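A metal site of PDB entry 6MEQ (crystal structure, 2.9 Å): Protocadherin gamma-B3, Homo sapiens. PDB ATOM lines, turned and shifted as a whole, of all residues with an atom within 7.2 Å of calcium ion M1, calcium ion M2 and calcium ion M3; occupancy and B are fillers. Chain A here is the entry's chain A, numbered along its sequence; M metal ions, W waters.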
ATOM      1  N   GLU A 114      10.127 -17.161 -15.501  1.00  0.00           N
ATOM      2  CA  GLU A 114      10.889 -16.948 -14.284  1.00  0.00           C
ATOM      3  C   GLU A 114      12.166 -17.785 -14.226  1.00  0.00           C
ATOM      4  O   GLU A 114      12.989 -17.537 -13.343  1.00  0.00           O
ATOM      5  CB  GLU A 114      10.010 -17.255 -13.063  1.00  0.00           C
ATOM      6  CG  GLU A 114       9.447 -18.653 -13.035  1.00  0.00           C
ATOM      7  CD  GLU A 114       8.610 -18.915 -11.801  1.00  0.00           C
ATOM      8  OE1 GLU A 114       8.586 -18.057 -10.892  1.00  0.00           O
ATOM      9  OE2 GLU A 114       7.959 -19.982 -11.740  1.00  0.00           O
ATOM     10  N   LEU A 170      13.768 -13.406 -11.519  1.00  0.00           N
ATOM     11  CA  LEU A 170      12.343 -13.145 -11.391  1.00  0.00           C
ATOM     12  C   LEU A 170      11.641 -14.298 -10.672  1.00  0.00           C
ATOM     13  O   LEU A 170      12.039 -15.460 -10.775  1.00  0.00           O
ATOM     14  CB  LEU A 170      11.707 -12.943 -12.768  1.00  0.00           C
ATOM     15  CG  LEU A 170      12.200 -11.737 -13.575  1.00  0.00           C
ATOM     16  CD1 LEU A 170      11.442 -11.628 -14.885  1.00  0.00           C
ATOM     17  CD2 LEU A 170      12.073 -10.455 -12.768  1.00  0.00           C
ATOM     18  N   ASP A 171      10.584 -13.951  -9.938  1.00  0.00           N
ATOM     19  CA  ASP A 171       9.806 -14.922  -9.169  1.00  0.00           C
ATOM     20  C   ASP A 171       8.337 -14.519  -9.255  1.00  0.00           C
ATOM     21  O   ASP A 171       7.950 -13.475  -8.725  1.00  0.00           O
ATOM     22  CB  ASP A 171      10.276 -14.988  -7.720  1.00  0.00           C
ATOM     23  CG  ASP A 171       9.637 -16.128  -6.944  1.00  0.00           C
ATOM     24  OD1 ASP A 171       8.900 -16.932  -7.558  1.00  0.00           O
ATOM     25  OD2 ASP A 171       9.872 -16.220  -5.716  1.00  0.00           O
ATOM     26  N   ARG A 172       7.530 -15.356  -9.926  1.00  0.00           N
ATOM     27  CA  ARG A 172       6.110 -15.045 -10.049  1.00  0.00           C
ATOM     28  C   ARG A 172       5.396 -15.171  -8.703  1.00  0.00           C
ATOM     29  O   ARG A 172       4.426 -14.453  -8.454  1.00  0.00           O
ATOM     30  CB  ARG A 172       5.465 -15.964 -11.081  1.00  0.00           C
ATOM     31  CG  ARG A 172       4.019 -15.608 -11.402  1.00  0.00           C
ATOM     32  CD  ARG A 172       3.321 -16.754 -12.110  1.00  0.00           C
ATOM     33  NE  ARG A 172       3.298 -17.959 -11.286  1.00  0.00           N
ATOM     34  CZ  ARG A 172       2.317 -18.270 -10.441  1.00  0.00           C
ATOM     35  NH1 ARG A 172       2.385 -19.391  -9.740  1.00  0.00           N
ATOM     36  NH2 ARG A 172       1.272 -17.461 -10.307  1.00  0.00           N
ATOM     37  N   GLU A 173       5.859 -16.078  -7.840  1.00  0.00           N
ATOM     38  CA  GLU A 173       5.239 -16.241  -6.529  1.00  0.00           C
ATOM     39  C   GLU A 173       5.464 -15.039  -5.626  1.00  0.00           C
ATOM     40  O   GLU A 173       4.778 -14.910  -4.605  1.00  0.00           O
ATOM     41  CB  GLU A 173       5.761 -17.510  -5.859  1.00  0.00           C
ATOM     42  CG  GLU A 173       5.116 -18.807  -6.348  1.00  0.00           C
ATOM     43  CD  GLU A 173       5.413 -19.104  -7.813  1.00  0.00           C
ATOM     44  OE1 GLU A 173       6.449 -18.636  -8.325  1.00  0.00           O
ATOM     45  OE2 GLU A 173       4.605 -19.815  -8.442  1.00  0.00           O
ATOM     46  N   GLU A 174       6.415 -14.174  -5.971  1.00  0.00           N
ATOM     47  CA  GLU A 174       6.680 -12.945  -5.206  1.00  0.00           C
ATOM     48  C   GLU A 174       6.120 -11.700  -5.879  1.00  0.00           C
ATOM     49  O   GLU A 174       5.521 -10.859  -5.210  1.00  0.00           O
ATOM     50  CB  GLU A 174       8.187 -12.784  -4.993  1.00  0.00           C
ATOM     51  CG  GLU A 174       8.561 -11.576  -4.140  1.00  0.00           C
ATOM     52  CD  GLU A 174       8.155 -11.724  -2.690  1.00  0.00           C
ATOM     53  OE1 GLU A 174       7.927 -12.871  -2.246  1.00  0.00           O
ATOM     54  OE2 GLU A 174       8.059 -10.695  -1.987  1.00  0.00           O
ATOM     55  N   ALA A 203       6.043 -15.286 -16.641  1.00  0.00           N
ATOM     56  CA  ALA A 203       5.449 -16.583 -16.926  1.00  0.00           C
ATOM     57  C   ALA A 203       5.818 -17.592 -15.843  1.00  0.00           C
ATOM     58  O   ALA A 203       6.907 -17.542 -15.269  1.00  0.00           O
ATOM     59  CB  ALA A 203       5.901 -17.099 -18.299  1.00  0.00           C
ATOM     60  N   ASP A 204       4.896 -18.516 -15.580  1.00  0.00           N
ATOM     61  CA  ASP A 204       5.055 -19.459 -14.479  1.00  0.00           C
ATOM     62  C   ASP A 204       5.818 -20.696 -14.938  1.00  0.00           C
ATOM     63  O   ASP A 204       5.561 -21.243 -16.008  1.00  0.00           O
ATOM     64  CB  ASP A 204       3.695 -19.879 -13.929  1.00  0.00           C
ATOM     65  CG  ASP A 204       3.821 -20.769 -12.706  1.00  0.00           C
ATOM     66  OD1 ASP A 204       4.367 -20.305 -11.684  1.00  0.00           O
ATOM     67  OD2 ASP A 204       3.369 -21.936 -12.762  1.00  0.00           O
ATOM     68  N   ALA A 205       6.771 -21.120 -14.106  1.00  0.00           N
ATOM     69  CA  ALA A 205       7.487 -22.369 -14.301  1.00  0.00           C
ATOM     70  C   ALA A 205       7.370 -23.203 -13.029  1.00  0.00           C
ATOM     71  O   ALA A 205       7.166 -22.671 -11.937  1.00  0.00           O
ATOM     72  CB  ALA A 205       8.959 -22.139 -14.659  1.00  0.00           C
ATOM     73  N   ASN A 206       7.508 -24.515 -13.191  1.00  0.00           N
ATOM     74  CA  ASN A 206       7.354 -25.451 -12.066  1.00  0.00           C
ATOM     75  C   ASN A 206       8.581 -25.350 -11.171  1.00  0.00           C
ATOM     76  O   ASN A 206       9.487 -26.186 -11.186  1.00  0.00           O
ATOM     77  CB  ASN A 206       7.145 -26.876 -12.574  1.00  0.00           C
ATOM     78  CG  ASN A 206       6.406 -27.735 -11.583  1.00  0.00           C
ATOM     79  OD1 ASN A 206       5.533 -27.264 -10.862  1.00  0.00           O
ATOM     80  ND2 ASN A 206       6.759 -29.014 -11.532  1.00  0.00           N
ATOM     81  N   ASP A 207       8.614 -24.278 -10.367  1.00  0.00           N
ATOM     82  CA  ASP A 207       9.724 -24.022  -9.446  1.00  0.00           C
ATOM     83  C   ASP A 207       9.360 -24.318  -7.998  1.00  0.00           C
ATOM     84  O   ASP A 207      10.005 -23.808  -7.081  1.00  0.00           O
ATOM     85  CB  ASP A 207      10.200 -22.575  -9.601  1.00  0.00           C
ATOM     86  CG  ASP A 207       9.124 -21.559  -9.237  1.00  0.00           C
ATOM     87  OD1 ASP A 207       7.929 -21.918  -9.296  1.00  0.00           O
ATOM     88  OD2 ASP A 207       9.479 -20.415  -8.895  1.00  0.00           O
ATOM     89  N   ASN A 208       8.327 -25.134  -7.766  1.00  0.00           N
ATOM     90  CA  ASN A 208       7.922 -25.487  -6.416  1.00  0.00           C
ATOM     91  C   ASN A 208       7.200 -26.830  -6.413  1.00  0.00           C
ATOM     92  O   ASN A 208       6.099 -26.939  -6.964  1.00  0.00           O
ATOM     93  CB  ASN A 208       7.029 -24.396  -5.824  1.00  0.00           C
ATOM     94  CG  ASN A 208       7.667 -23.693  -4.646  1.00  0.00           C
ATOM     95  OD1 ASN A 208       8.431 -24.284  -3.886  1.00  0.00           O
ATOM     96  ND2 ASN A 208       7.372 -22.404  -4.491  1.00  0.00           N
ATOM     97  N   PRO A 209       7.779 -27.850  -5.807  1.00  0.00           N
ATOM     98  CA  PRO A 209       7.130 -29.161  -5.756  1.00  0.00           C
ATOM     99  C   PRO A 209       6.009 -29.169  -4.735  1.00  0.00           C
ATOM    100  O   PRO A 209       5.936 -28.272  -3.882  1.00  0.00           O
ATOM    101  CB  PRO A 209       8.263 -30.109  -5.345  1.00  0.00           C
ATOM    102  CG  PRO A 209       9.178 -29.246  -4.546  1.00  0.00           C
ATOM    103  CD  PRO A 209       9.113 -27.873  -5.172  1.00  0.00           C
ATOM    104  N   PRO A 210       5.101 -30.152  -4.796  1.00  0.00           N
ATOM    105  CA  PRO A 210       4.037 -30.228  -3.789  1.00  0.00           C
ATOM    106  C   PRO A 210       4.595 -30.465  -2.397  1.00  0.00           C
ATOM    107  O   PRO A 210       5.640 -31.115  -2.222  1.00  0.00           O
ATOM    108  CB  PRO A 210       3.188 -31.418  -4.262  1.00  0.00           C
ATOM    109  CG  PRO A 210       3.492 -31.542  -5.718  1.00  0.00           C
ATOM    110  CD  PRO A 210       4.926 -31.148  -5.869  1.00  0.00           C
ATOM    111  N   ILE A 237       0.018 -28.759  -0.886  1.00  0.00           N
ATOM    112  CA  ILE A 237      -0.030 -27.370  -1.311  1.00  0.00           C
ATOM    113  C   ILE A 237       1.012 -27.153  -2.393  1.00  0.00           C
ATOM    114  O   ILE A 237       2.173 -27.563  -2.236  1.00  0.00           O
ATOM    115  CB  ILE A 237       0.193 -26.407  -0.129  1.00  0.00           C
ATOM    116  CG1 ILE A 237      -0.840 -26.671   0.972  1.00  0.00           C
ATOM    117  CG2 ILE A 237       0.119 -24.964  -0.591  1.00  0.00           C
ATOM    118  CD1 ILE A 237      -0.695 -25.772   2.182  1.00  0.00           C
ATOM    119  N   ASP A 238       0.600 -26.514  -3.492  1.00  0.00           N
ATOM    120  CA  ASP A 238       1.489 -26.193  -4.602  1.00  0.00           C
ATOM    121  C   ASP A 238       1.331 -24.708  -4.918  1.00  0.00           C
ATOM    122  O   ASP A 238       0.229 -24.247  -5.186  1.00  0.00           O
ATOM    123  CB  ASP A 238       1.169 -27.047  -5.822  1.00  0.00           C
ATOM    124  CG  ASP A 238       2.339 -27.150  -6.792  1.00  0.00           C
ATOM    125  OD1 ASP A 238       3.109 -26.170  -6.905  1.00  0.00           O
ATOM    126  OD2 ASP A 238       2.498 -28.215  -7.422  1.00  0.00           O
ATOM    127  N   MET A 239       2.443 -23.974  -4.883  1.00  0.00           N
ATOM    128  CA  MET A 239       2.431 -22.531  -5.060  1.00  0.00           C
ATOM    129  C   MET A 239       2.478 -22.100  -6.518  1.00  0.00           C
ATOM    130  O   MET A 239       2.570 -20.903  -6.794  1.00  0.00           O
ATOM    131  CB  MET A 239       3.607 -21.895  -4.298  1.00  0.00           C
ATOM    132  CG  MET A 239       3.571 -22.118  -2.800  1.00  0.00           C
ATOM    133  SD  MET A 239       2.104 -21.397  -2.027  1.00  0.00           S
ATOM    134  CE  MET A 239       2.386 -21.819  -0.308  1.00  0.00           C
ATOM    135  N   ASP A 240       2.415 -23.040  -7.454  1.00  0.00           N
ATOM    136  CA  ASP A 240       2.506 -22.722  -8.874  1.00  0.00           C
ATOM    137  C   ASP A 240       1.105 -22.483  -9.437  1.00  0.00           C
ATOM    138  O   ASP A 240       0.118 -22.414  -8.705  1.00  0.00           O
ATOM    139  CB  ASP A 240       3.252 -23.832  -9.610  1.00  0.00           C
ATOM    140  CG  ASP A 240       4.700 -23.942  -9.180  1.00  0.00           C
ATOM    141  OD1 ASP A 240       5.308 -22.896  -8.900  1.00  0.00           O
ATOM    142  OD2 ASP A 240       5.227 -25.074  -9.126  1.00  0.00           O
ATOM    143  N   GLU A 241       1.018 -22.330 -10.762  1.00  0.00           N
ATOM    144  CA  GLU A 241      -0.222 -21.958 -11.424  1.00  0.00           C
ATOM    145  C   GLU A 241      -0.442 -22.835 -12.645  1.00  0.00           C
ATOM    146  O   GLU A 241       0.493 -23.131 -13.388  1.00  0.00           O
ATOM    147  CB  GLU A 241      -0.192 -20.483 -11.858  1.00  0.00           C
ATOM    148  CG  GLU A 241      -1.441 -20.009 -12.586  1.00  0.00           C
ATOM    149  CD  GLU A 241      -1.303 -18.586 -13.112  1.00  0.00           C
ATOM    150  OE1 GLU A 241      -0.218 -17.989 -12.935  1.00  0.00           O
ATOM    151  OE2 GLU A 241      -2.276 -18.073 -13.701  1.00  0.00           O
ATOM    152  N   ILE A 243      -1.183 -26.058 -14.925  1.00  0.00           N
ATOM    153  CA  ILE A 243      -0.874 -27.483 -14.878  1.00  0.00           C
ATOM    154  C   ILE A 243       0.167 -27.781 -13.816  1.00  0.00           C
ATOM    155  O   ILE A 243       0.192 -28.880 -13.232  1.00  0.00           O
ATOM    156  CB  ILE A 243      -0.435 -27.973 -16.280  1.00  0.00           C
ATOM    157  CG1 ILE A 243      -0.137 -29.472 -16.264  1.00  0.00           C
ATOM    158  CG2 ILE A 243       0.784 -27.192 -16.758  1.00  0.00           C
ATOM    159  CD1 ILE A 243      -1.324 -30.335 -15.896  1.00  0.00           C
ATOM    160  N   ASN A 244       1.053 -26.822 -13.525  1.00  0.00           N
ATOM    161  CA  ASN A 244       2.071 -26.986 -12.506  1.00  0.00           C
ATOM    162  C   ASN A 244       1.504 -26.950 -11.093  1.00  0.00           C
ATOM    163  O   ASN A 244       2.282 -27.081 -10.131  1.00  0.00           O
ATOM    164  CB  ASN A 244       3.147 -25.914 -12.656  1.00  0.00           C
ATOM    165  CG  ASN A 244       3.792 -25.928 -14.028  1.00  0.00           C
ATOM    166  OD1 ASN A 244       3.890 -26.980 -14.673  1.00  0.00           O
ATOM    167  ND2 ASN A 244       4.239 -24.764 -14.483  1.00  0.00           N
ATOM    168  N   ALA A 245       0.197 -26.776 -10.931  1.00  0.00           N
ATOM    169  CA  ALA A 245      -0.438 -26.739  -9.622  1.00  0.00           C
ATOM    170  C   ALA A 245      -1.414 -27.881  -9.371  1.00  0.00           C
ATOM    171  O   ALA A 245      -1.734 -28.159  -8.209  1.00  0.00           O
ATOM    172  CB  ALA A 245      -1.176 -25.408  -9.400  1.00  0.00           C
ATOM    173  N   GLU A 246      -1.899 -28.546 -10.426  1.00  0.00           N
ATOM    174  CA  GLU A 246      -2.809 -29.670 -10.237  1.00  0.00           C
ATOM    175  C   GLU A 246      -2.070 -30.848  -9.628  1.00  0.00           C
ATOM    176  O   GLU A 246      -1.024 -31.279 -10.142  1.00  0.00           O
ATOM    177  CB  GLU A 246      -3.435 -30.059 -11.578  1.00  0.00           C
ATOM    178  CG  GLU A 246      -4.204 -28.933 -12.259  1.00  0.00           C
ATOM    179  CD  GLU A 246      -4.749 -29.337 -13.609  1.00  0.00           C
ATOM    180  OE1 GLU A 246      -4.561 -30.502 -14.003  1.00  0.00           O
ATOM    181  OE2 GLU A 246      -5.379 -28.491 -14.274  1.00  0.00           O
ATOM    182  N   ILE A 247      -2.602 -31.384  -8.529  1.00  0.00           N
ATOM    183  CA  ILE A 247      -1.952 -32.439  -7.762  1.00  0.00           C
ATOM    184  C   ILE A 247      -2.813 -33.690  -7.823  1.00  0.00           C
ATOM    185  O   ILE A 247      -4.042 -33.611  -7.664  1.00  0.00           O
ATOM    186  CB  ILE A 247      -1.711 -32.007  -6.308  1.00  0.00           C
ATOM    187  CG1 ILE A 247      -0.894 -30.720  -6.258  1.00  0.00           C
ATOM    188  CG2 ILE A 247      -1.002 -33.117  -5.535  1.00  0.00           C
ATOM    189  CD1 ILE A 247      -0.641 -30.203  -4.861  1.00  0.00           C
ATOM    190  N   ASP A 293       2.540 -33.634  -9.753  1.00  0.00           N
ATOM    191  CA  ASP A 293       1.981 -32.457 -10.407  1.00  0.00           C
ATOM    192  C   ASP A 293       2.208 -32.512 -11.912  1.00  0.00           C
ATOM    193  O   ASP A 293       2.474 -33.588 -12.455  1.00  0.00           O
ATOM    194  CB  ASP A 293       2.590 -31.172  -9.823  1.00  0.00           C
ATOM    195  CG  ASP A 293       4.112 -31.131  -9.940  1.00  0.00           C
ATOM    196  OD1 ASP A 293       4.702 -32.138 -10.391  1.00  0.00           O
ATOM    197  OD2 ASP A 293       4.705 -30.098  -9.589  1.00  0.00           O
ATOM    198  N   GLY A 294       2.083 -31.372 -12.584  1.00  0.00           N
ATOM    199  CA  GLY A 294       2.273 -31.342 -14.024  1.00  0.00           C
ATOM    200  C   GLY A 294       3.714 -31.506 -14.447  1.00  0.00           C
ATOM    201  O   GLY A 294       4.002 -32.125 -15.476  1.00  0.00           O
ATOM    202  N   GLY A 295       4.647 -30.969 -13.665  1.00  0.00           N
ATOM    203  CA  GLY A 295       6.061 -31.062 -13.986  1.00  0.00           C
ATOM    204  C   GLY A 295       6.724 -32.292 -13.415  1.00  0.00           C
ATOM    205  O   GLY A 295       7.953 -32.348 -13.305  1.00  0.00           O
ATOM    206  N   HIS A 297       6.910 -33.355 -10.432  1.00  0.00           N
ATOM    207  CA  HIS A 297       7.527 -33.193  -9.128  1.00  0.00           C
ATOM    208  C   HIS A 297       6.799 -34.059  -8.110  1.00  0.00           C
ATOM    209  O   HIS A 297       5.568 -34.005  -7.994  1.00  0.00           O
ATOM    210  CB  HIS A 297       7.510 -31.726  -8.693  1.00  0.00           C
ATOM    211  CG  HIS A 297       8.586 -30.894  -9.319  1.00  0.00           C
ATOM    212  ND1 HIS A 297       9.486 -31.407 -10.231  1.00  0.00           N
ATOM    213  CD2 HIS A 297       8.913 -29.593  -9.153  1.00  0.00           C
ATOM    214  CE1 HIS A 297      10.319 -30.454 -10.609  1.00  0.00           C
ATOM    215  NE2 HIS A 297       9.991 -29.342  -9.976  1.00  0.00           N
HETATM  216 CA    CA M   1       6.199 -20.539 -10.148  1.00  0.00          CA
HETATM  217 CA    CA M   2       4.428 -27.417  -8.729  1.00  0.00          CA
HETATM  218 CA    CA M   3       8.379 -19.307  -6.949  1.00  0.00          CA
HETATM  219  O   HOH W   1      10.524 -19.203  -5.663  1.00  0.00           O
HETATM  220  O   HOH W   2      11.488 -18.864  -8.247  1.00  0.00           O
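OD2 of Asp 204 sits at hydrogen-bond distance from ND2 of Asn 244, 3.4 Å away. OD1 of Asp 293 lies close to N of Gly 295 (3.5 Å). The backbone NH (N) of Glu 114 is in hydrogen-bond range of the backbone carbonyl oxygen (O) of Ala 203. The guanidinium group (NH1) of Arg 172 lies close to the side-chain carboxylate (OE2) of Glu 173 (2.6 Å). The backbone NH (N) of Glu 241 sits at hydrogen-bond distance from the side-chain carboxylate (OD2) of Asp 204, at 3.1 Å. O of Asn 206 lies within hydrogen-bond range of NE2 of His 297 (3.4 Å). N of Ala 205 sits close to OE2 of Glu 114 (2.9 Å). NE of Arg 172 sits close to OD1 of Asp 204, at 2.6 Å.
The nearest printed residue that does not touch calcium ion M1 is Arg 172 (4.004 Å).
Within 4 Å of calcium ion M2: Asn 206, Asn 208, Asp 238, Asp 240, Asn 244 and Asp 293. Along chain A the residues within 4 Å of calcium ion M2 span positions 206 to 293. The nearest printed residue that does not touch calcium ion M2 is Pro 209 (4.4 Å).
The nearest printed residue that does not touch calcium ion M3 is Asn 208 (4.1 Å).
Calcium ion M1 is bound by the side-chain carboxylate (OD1) of Asp 207, the side-chain carboxylate (OD1) of Asp 204, the side-chain carboxylate (OE2) of Glu 114, the side-chain carboxylate (OE2) of Glu 173, the side-chain carboxylate (OE1) of Glu 173 and the side-chain carboxylate (OD1) of Asp 240. Slightly farther from calcium ion M1 lies the backbone carbonyl oxygen (O) of Ala 205 (2.9 Å).
Calcium ion M2 is bound by the side-chain amide oxygen (OD1) of Asn 206, the side-chain carboxylate (OD2) of Asp 238, the backbone carbonyl oxygen (O) of Asn 208, the side-chain carboxylate (OD2) of Asp 240, the side-chain carboxylate (OD1) of Asp 238, the backbone carbonyl oxygen (O) of Asn 244 and the side-chain carboxylate (OD2) of Asp 293. Calcium ion M2 has seven donor atoms within binding distance.
Calcium ion M3 is bound by the side-chain carboxylate of Glu 173 (2.5 Å), the side-chain carboxylate of Asp 207 (2.5 Å), water W1 (2.5 Å) and the side-chain carboxylate of Asp 171 (2.5 Å). Calcium ion M3 has four donor atoms within binding distance.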
